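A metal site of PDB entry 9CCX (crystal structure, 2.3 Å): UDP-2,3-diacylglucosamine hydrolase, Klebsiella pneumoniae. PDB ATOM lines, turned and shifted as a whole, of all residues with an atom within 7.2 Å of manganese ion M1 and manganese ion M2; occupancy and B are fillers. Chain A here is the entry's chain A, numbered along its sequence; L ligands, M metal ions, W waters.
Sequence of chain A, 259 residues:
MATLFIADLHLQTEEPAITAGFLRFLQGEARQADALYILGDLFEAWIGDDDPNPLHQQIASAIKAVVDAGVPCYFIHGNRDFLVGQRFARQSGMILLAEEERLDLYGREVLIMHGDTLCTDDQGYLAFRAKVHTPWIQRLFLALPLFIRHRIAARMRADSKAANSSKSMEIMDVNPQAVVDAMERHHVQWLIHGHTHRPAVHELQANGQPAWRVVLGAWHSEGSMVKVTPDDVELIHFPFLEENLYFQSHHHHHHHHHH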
ATOM      1  N   ALA A   7      15.549   6.855 -26.540  1.00  0.00           N
ATOM      2  CA  ALA A   7      16.960   6.886 -26.180  1.00  0.00           C
ATOM      3  C   ALA A   7      17.575   8.129 -26.792  1.00  0.00           C
ATOM      4  O   ALA A   7      17.009   8.756 -27.688  1.00  0.00           O
ATOM      5  CB  ALA A   7      17.711   5.638 -26.660  1.00  0.00           C
ATOM      6  N   ASP A   8      18.748   8.486 -26.257  1.00  0.00           N
ATOM      7  CA  ASP A   8      19.656   9.406 -26.911  1.00  0.00           C
ATOM      8  C   ASP A   8      19.046  10.795 -27.035  1.00  0.00           C
ATOM      9  O   ASP A   8      19.120  11.426 -28.088  1.00  0.00           O
ATOM     10  CB  ASP A   8      20.071   8.877 -28.285  1.00  0.00           C
ATOM     11  CG  ASP A   8      20.963   7.653 -28.181  1.00  0.00           C
ATOM     12  OD1 ASP A   8      22.088   7.766 -27.679  1.00  0.00           O
ATOM     13  OD2 ASP A   8      20.537   6.552 -28.578  1.00  0.00           O
ATOM     14  N   LEU A   9      18.422  11.255 -25.949  1.00  0.00           N
ATOM     15  CA  LEU A   9      17.857  12.597 -25.876  1.00  0.00           C
ATOM     16  C   LEU A   9      18.941  13.638 -25.613  1.00  0.00           C
ATOM     17  O   LEU A   9      18.844  14.774 -26.103  1.00  0.00           O
ATOM     18  CB  LEU A   9      16.818  12.644 -24.772  1.00  0.00           C
ATOM     19  CG  LEU A   9      15.441  12.073 -25.104  1.00  0.00           C
ATOM     20  CD1 LEU A   9      15.459  10.545 -24.953  1.00  0.00           C
ATOM     21  CD2 LEU A   9      14.371  12.725 -24.214  1.00  0.00           C
ATOM     22  N   HIS A  10      19.965  13.280 -24.817  1.00  0.00           N
ATOM     23  CA  HIS A  10      21.063  14.185 -24.490  1.00  0.00           C
ATOM     24  C   HIS A  10      20.571  15.507 -23.891  1.00  0.00           C
ATOM     25  O   HIS A  10      21.003  16.588 -24.287  1.00  0.00           O
ATOM     26  CB  HIS A  10      21.933  14.449 -25.723  1.00  0.00           C
ATOM     27  CG  HIS A  10      22.316  13.203 -26.443  1.00  0.00           C
ATOM     28  ND1 HIS A  10      21.775  12.847 -27.658  1.00  0.00           N
ATOM     29  CD2 HIS A  10      23.183  12.216 -26.117  1.00  0.00           C
ATOM     30  CE1 HIS A  10      22.295  11.703 -28.053  1.00  0.00           C
ATOM     31  NE2 HIS A  10      23.150  11.287 -27.129  1.00  0.00           N
ATOM     32  N   LEU A  39      16.550   3.774 -23.040  1.00  0.00           N
ATOM     33  CA  LEU A  39      17.744   2.952 -23.283  1.00  0.00           C
ATOM     34  C   LEU A  39      19.022   3.786 -23.335  1.00  0.00           C
ATOM     35  O   LEU A  39      19.850   3.619 -24.224  1.00  0.00           O
ATOM     36  CB  LEU A  39      17.561   2.153 -24.573  1.00  0.00           C
ATOM     37  CG  LEU A  39      16.258   1.345 -24.694  1.00  0.00           C
ATOM     38  CD1 LEU A  39      16.257   0.463 -25.944  1.00  0.00           C
ATOM     39  CD2 LEU A  39      16.010   0.518 -23.453  1.00  0.00           C
ATOM     40  N   GLY A  40      19.210   4.682 -22.378  1.00  0.00           N
ATOM     41  CA  GLY A  40      20.490   5.335 -22.202  1.00  0.00           C
ATOM     42  C   GLY A  40      20.585   6.667 -22.933  1.00  0.00           C
ATOM     43  O   GLY A  40      19.858   6.946 -23.892  1.00  0.00           O
ATOM     44  N   ASP A  41      21.536   7.491 -22.464  1.00  0.00           N
ATOM     45  CA  ASP A  41      21.790   8.831 -23.001  1.00  0.00           C
ATOM     46  C   ASP A  41      20.577   9.746 -22.815  1.00  0.00           C
ATOM     47  O   ASP A  41      20.276  10.597 -23.673  1.00  0.00           O
ATOM     48  CB  ASP A  41      22.216   8.809 -24.480  1.00  0.00           C
ATOM     49  CG  ASP A  41      23.682   8.421 -24.688  1.00  0.00           C
ATOM     50  OD1 ASP A  41      24.372   8.081 -23.686  1.00  0.00           O
ATOM     51  OD2 ASP A  41      24.142   8.461 -25.855  1.00  0.00           O
ATOM     52  N   GLU A  44      22.978  14.574 -21.428  1.00  0.00           N
ATOM     53  CA  GLU A  44      24.236  14.770 -22.142  1.00  0.00           C
ATOM     54  C   GLU A  44      25.453  14.483 -21.262  1.00  0.00           C
ATOM     55  O   GLU A  44      26.529  14.150 -21.783  1.00  0.00           O
ATOM     56  CB  GLU A  44      24.305  16.198 -22.709  1.00  0.00           C
ATOM     57  CG  GLU A  44      25.664  16.607 -23.278  1.00  0.00           C
ATOM     58  CD  GLU A  44      25.914  16.032 -24.663  1.00  0.00           C
ATOM     59  OE1 GLU A  44      25.142  15.137 -25.087  1.00  0.00           O
ATOM     60  OE2 GLU A  44      26.906  16.440 -25.314  1.00  0.00           O
ATOM     61  N   GLY A  78      23.409   4.800 -20.634  1.00  0.00           N
ATOM     62  CA  GLY A  78      24.095   5.075 -21.874  1.00  0.00           C
ATOM     63  C   GLY A  78      25.565   5.327 -21.624  1.00  0.00           C
ATOM     64  O   GLY A  78      26.066   5.243 -20.507  1.00  0.00           O
ATOM     65  N   ASN A  79      26.279   5.630 -22.716  1.00  0.00           N
ATOM     66  CA  ASN A  79      27.685   5.951 -22.543  1.00  0.00           C
ATOM     67  C   ASN A  79      27.887   7.342 -21.953  1.00  0.00           C
ATOM     68  O   ASN A  79      28.926   7.588 -21.339  1.00  0.00           O
ATOM     69  CB  ASN A  79      28.449   5.813 -23.871  1.00  0.00           C
ATOM     70  CG  ASN A  79      27.987   6.796 -24.931  1.00  0.00           C
ATOM     71  OD1 ASN A  79      26.846   6.747 -25.387  1.00  0.00           O
ATOM     72  ND2 ASN A  79      28.898   7.663 -25.371  1.00  0.00           N
ATOM     73  N   ARG A  80      26.901   8.228 -22.090  1.00  0.00           N
ATOM     74  CA  ARG A  80      27.031   9.572 -21.515  1.00  0.00           C
ATOM     75  C   ARG A  80      26.609   9.641 -20.055  1.00  0.00           C
ATOM     76  O   ARG A  80      27.223  10.367 -19.273  1.00  0.00           O
ATOM     77  CB  ARG A  80      26.207  10.589 -22.326  1.00  0.00           C
ATOM     78  CG  ARG A  80      26.503  10.617 -23.809  1.00  0.00           C
ATOM     79  CD  ARG A  80      27.938  11.042 -24.102  1.00  0.00           C
ATOM     80  NE  ARG A  80      28.209  12.374 -23.583  1.00  0.00           N
ATOM     81  CZ  ARG A  80      29.291  13.085 -23.874  1.00  0.00           C
ATOM     82  NH1 ARG A  80      30.221  12.625 -24.700  1.00  0.00           N
ATOM     83  NH2 ARG A  80      29.447  14.279 -23.315  1.00  0.00           N
ATOM     84  N   ASP A  81      25.559   8.906 -19.658  1.00  0.00           N
ATOM     85  CA  ASP A  81      24.998   9.040 -18.312  1.00  0.00           C
ATOM     86  C   ASP A  81      25.132   7.750 -17.499  1.00  0.00           C
ATOM     87  O   ASP A  81      24.255   7.403 -16.698  1.00  0.00           O
ATOM     88  CB  ASP A  81      23.533   9.506 -18.384  1.00  0.00           C
ATOM     89  CG  ASP A  81      22.703   8.745 -19.449  1.00  0.00           C
ATOM     90  OD1 ASP A  81      23.141   7.685 -19.954  1.00  0.00           O
ATOM     91  OD2 ASP A  81      21.602   9.231 -19.773  1.00  0.00           O
ATOM     92  N   HIS A 114      21.676  -0.350 -24.678  1.00  0.00           N
ATOM     93  CA  HIS A 114      21.986   0.968 -25.227  1.00  0.00           C
ATOM     94  C   HIS A 114      22.590   0.860 -26.622  1.00  0.00           C
ATOM     95  O   HIS A 114      22.296   1.681 -27.498  1.00  0.00           O
ATOM     96  CB  HIS A 114      22.943   1.739 -24.309  1.00  0.00           C
ATOM     97  CG  HIS A 114      23.271   3.110 -24.822  1.00  0.00           C
ATOM     98  ND1 HIS A 114      22.312   4.075 -25.034  1.00  0.00           N
ATOM     99  CD2 HIS A 114      24.452   3.662 -25.212  1.00  0.00           C
ATOM    100  CE1 HIS A 114      22.883   5.171 -25.499  1.00  0.00           C
ATOM    101  NE2 HIS A 114      24.181   4.945 -25.635  1.00  0.00           N
ATOM    102  N   GLY A 115      23.435  -0.147 -26.848  1.00  0.00           N
ATOM    103  CA  GLY A 115      24.047  -0.383 -28.139  1.00  0.00           C
ATOM    104  C   GLY A 115      25.519  -0.024 -28.227  1.00  0.00           C
ATOM    105  O   GLY A 115      26.155  -0.366 -29.231  1.00  0.00           O
ATOM    106  N   ASP A 116      26.098   0.633 -27.231  1.00  0.00           N
ATOM    107  CA  ASP A 116      27.492   1.026 -27.395  1.00  0.00           C
ATOM    108  C   ASP A 116      28.419  -0.186 -27.345  1.00  0.00           C
ATOM    109  O   ASP A 116      29.491  -0.168 -27.969  1.00  0.00           O
ATOM    110  CB  ASP A 116      27.909   2.091 -26.369  1.00  0.00           C
ATOM    111  CG  ASP A 116      27.817   1.603 -24.939  1.00  0.00           C
ATOM    112  OD1 ASP A 116      26.779   1.002 -24.567  1.00  0.00           O
ATOM    113  OD2 ASP A 116      28.792   1.823 -24.180  1.00  0.00           O
ATOM    114  N   TYR A 125      37.188   3.757 -28.243  1.00  0.00           N
ATOM    115  CA  TYR A 125      36.059   3.879 -27.335  1.00  0.00           C
ATOM    116  C   TYR A 125      36.055   2.769 -26.298  1.00  0.00           C
ATOM    117  O   TYR A 125      35.790   3.015 -25.111  1.00  0.00           O
ATOM    118  CB  TYR A 125      34.730   3.891 -28.090  1.00  0.00           C
ATOM    119  CG  TYR A 125      33.572   3.770 -27.123  1.00  0.00           C
ATOM    120  CD1 TYR A 125      33.326   4.782 -26.202  1.00  0.00           C
ATOM    121  CD2 TYR A 125      32.722   2.673 -27.136  1.00  0.00           C
ATOM    122  CE1 TYR A 125      32.291   4.696 -25.283  1.00  0.00           C
ATOM    123  CE2 TYR A 125      31.671   2.576 -26.237  1.00  0.00           C
ATOM    124  CZ  TYR A 125      31.465   3.594 -25.311  1.00  0.00           C
ATOM    125  OH  TYR A 125      30.440   3.515 -24.404  1.00  0.00           O
ATOM    126  N   GLY A 194      19.877   1.973 -29.082  1.00  0.00           N
ATOM    127  CA  GLY A 194      20.120   3.307 -29.606  1.00  0.00           C
ATOM    128  C   GLY A 194      21.594   3.538 -29.871  1.00  0.00           C
ATOM    129  O   GLY A 194      22.226   2.782 -30.621  1.00  0.00           O
ATOM    130  N   HIS A 195      22.133   4.604 -29.268  1.00  0.00           N
ATOM    131  CA  HIS A 195      23.546   4.966 -29.292  1.00  0.00           C
ATOM    132  C   HIS A 195      24.086   5.404 -30.646  1.00  0.00           C
ATOM    133  O   HIS A 195      24.798   6.403 -30.715  1.00  0.00           O
ATOM    134  CB  HIS A 195      24.427   3.828 -28.794  1.00  0.00           C
ATOM    135  CG  HIS A 195      25.888   4.145 -28.899  1.00  0.00           C
ATOM    136  ND1 HIS A 195      26.482   5.140 -28.153  1.00  0.00           N
ATOM    137  CD2 HIS A 195      26.853   3.627 -29.691  1.00  0.00           C
ATOM    138  CE1 HIS A 195      27.765   5.205 -28.468  1.00  0.00           C
ATOM    139  NE2 HIS A 195      28.013   4.303 -29.394  1.00  0.00           N
ATOM    140  N   THR A 196      23.797   4.652 -31.721  1.00  0.00           N
ATOM    141  CA  THR A 196      24.364   5.016 -33.025  1.00  0.00           C
ATOM    142  C   THR A 196      23.678   6.198 -33.684  1.00  0.00           C
ATOM    143  O   THR A 196      24.252   6.756 -34.628  1.00  0.00           O
ATOM    144  CB  THR A 196      24.336   3.833 -33.988  1.00  0.00           C
ATOM    145  OG1 THR A 196      22.970   3.448 -34.235  1.00  0.00           O
ATOM    146  CG2 THR A 196      25.155   2.661 -33.431  1.00  0.00           C
ATOM    147  N   HIS A 197      22.480   6.585 -33.233  1.00  0.00           N
ATOM    148  CA  HIS A 197      21.769   7.729 -33.802  1.00  0.00           C
ATOM    149  C   HIS A 197      21.380   7.503 -35.269  1.00  0.00           C
ATOM    150  O   HIS A 197      21.215   8.457 -36.035  1.00  0.00           O
ATOM    151  CB  HIS A 197      22.583   9.036 -33.690  1.00  0.00           C
ATOM    152  CG  HIS A 197      22.941   9.431 -32.283  1.00  0.00           C
ATOM    153  ND1 HIS A 197      23.613  10.603 -32.004  1.00  0.00           N
ATOM    154  CD2 HIS A 197      22.700   8.837 -31.090  1.00  0.00           C
ATOM    155  CE1 HIS A 197      23.798  10.698 -30.695  1.00  0.00           C
ATOM    156  NE2 HIS A 197      23.248   9.644 -30.123  1.00  0.00           N
ATOM    157  N   ALA A 218      18.191   9.831 -32.273  1.00  0.00           N
ATOM    158  CA  ALA A 218      18.537  10.890 -31.337  1.00  0.00           C
ATOM    159  C   ALA A 218      17.570  12.057 -31.497  1.00  0.00           C
ATOM    160  O   ALA A 218      17.021  12.282 -32.587  1.00  0.00           O
ATOM    161  CB  ALA A 218      19.965  11.385 -31.574  1.00  0.00           C
HETATM  162  C1  LIG L   1      31.240  12.217 -20.235  1.00  0.00           C
HETATM  163  C2  LIG L   1      30.898  10.344 -21.715  1.00  0.00           C
HETATM  164  C3  LIG L   1      32.741  11.895 -22.094  1.00  0.00           C
HETATM  165  C4  LIG L   1      33.690  11.032 -24.150  1.00  0.00           C
HETATM  166  C5  LIG L   1      32.259   8.902 -24.287  1.00  0.00           C
HETATM  167  C6  LIG L   1      32.998   8.414 -25.528  1.00  0.00           C
HETATM  168  C7  LIG L   1      36.204   9.237 -14.271  1.00  0.00           C
HETATM  169  C8  LIG L   1      37.694   9.499 -14.122  1.00  0.00           C
HETATM  170  C9  LIG L   1      34.257   7.917 -13.850  1.00  0.00           C
HETATM  171  C10 LIG L   1      34.057   9.858 -15.081  1.00  0.00           C
HETATM  172  C11 LIG L   1      33.686  12.086 -16.209  1.00  0.00           C
HETATM  173  C12 LIG L   1      33.047  12.522 -17.513  1.00  0.00           C
HETATM  174  C13 LIG L   1      31.131  11.103 -17.051  1.00  0.00           C
HETATM  175  C14 LIG L   1      31.776  10.685 -15.733  1.00  0.00           C
HETATM  176  C15 LIG L   1      30.512  11.069 -20.592  1.00  0.00           C
HETATM  177  C16 LIG L   1      32.013  10.752 -22.464  1.00  0.00           C
HETATM  178  C17 LIG L   1      32.362  12.635 -20.965  1.00  0.00           C
HETATM  179  C18 LIG L   1      33.892  12.078 -23.091  1.00  0.00           C
HETATM  180  C19 LIG L   1      35.409  10.121 -14.971  1.00  0.00           C
HETATM  181  C20 LIG L   1      35.615   8.112 -13.696  1.00  0.00           C
HETATM  182  F1  LIG L   1      38.337   8.974 -15.186  1.00  0.00           F
HETATM  183  F2  LIG L   1      37.968  10.850 -14.079  1.00  0.00           F
HETATM  184  F3  LIG L   1      38.124   8.900 -12.975  1.00  0.00           F
HETATM  185  N1  LIG L   1      33.522   8.788 -14.521  1.00  0.00           N
HETATM  186  N2  LIG L   1      33.223  10.763 -15.822  1.00  0.00           N
HETATM  187  N3  LIG L   1      31.584  12.406 -17.499  1.00  0.00           N
HETATM  188  N4  LIG L   1      32.643  10.164 -23.681  1.00  0.00           N
HETATM  189  O1  LIG L   1      31.040  14.583 -18.905  1.00  0.00           O
HETATM  190  O2  LIG L   1      29.282  13.097 -18.550  1.00  0.00           O
HETATM  191  O3  LIG L   1      31.367   8.273 -23.818  1.00  0.00           O
HETATM  192  S1  LIG L   1      30.729  13.146 -18.771  1.00  0.00           S
HETATM  193 MN    MN M   1      25.323   6.651 -26.677  1.00  0.00          MN
HETATM  194 MN    MN M   2      23.607   9.174 -27.888  1.00  0.00          MN
HETATM  195  O   HOH W   1      25.306   7.920 -28.428  1.00  0.00           O
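An oxygen (O3) of the ligand sits at hydrogen-bond distance from the side-chain amide nitrogen (ND2) of Asn 79 (3.0 Å).
A ring nitrogen (ND1) of His 114 sits at hydrogen-bond distance from the backbone carbonyl oxygen (O) of Leu 39, 2.6 Å away. The backbone NH of Leu 9 sits at hydrogen-bond distance from the backbone carbonyl oxygen of Asp 41, 3.0 Å away. The side-chain carboxylate (OD2) of Asp 8 lies within hydrogen-bond range of the backbone NH (N) of His 195 (2.6 Å). The side-chain carboxylate (OD1) of Asp 41 lies within hydrogen-bond range of the backbone NH (N) of Arg 80, at 3.0 Å. The backbone NH (N) of Asp 41 is in hydrogen-bond range of the side-chain carboxylate (OD1) of Asp 81, at 3.0 Å. N of Gly 194 sits at hydrogen-bond distance from O of His 114, at 2.9 Å. The backbone NH of Asp 8 is in hydrogen-bond range of the backbone carbonyl oxygen of Gly 40.
Five residues have an atom within 4 Å of manganese ion M1: Asp 8, Asp 41, Asn 79, His 114 and His 195.
Four residues have an atom within 4 Å of manganese ion M2: Asp 8, His 10, Asp 41 and His 197. The nearest printed residue that does not touch manganese ion M2 is His 195 (4.1 Å).
Manganese ion M1 is bound by OD1 of Asn 79, 2.0 Å away. Water W1 is bound to manganese ion M1, at 2.2 Å. A ring nitrogen (NE2) of His 114 is bound to manganese ion M1 (2.3 Å). OD2 of Asp 41 binds manganese ion M1. A ring nitrogen (ND1) of His 195 binds manganese ion M1 (2.4 Å).
Manganese ion M2 is bound by the side-chain carboxylate of Asp 8 (2.1 Å), water W1 (2.2 Å), the side-chain carboxylate of Asp 41 (2.2 Å), a ring nitrogen (NE2) of His 10 (2.3 Å) and a ring nitrogen (NE2) of His 197 (2.3 Å). Manganese ion M2 has five donor atoms within binding distance.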
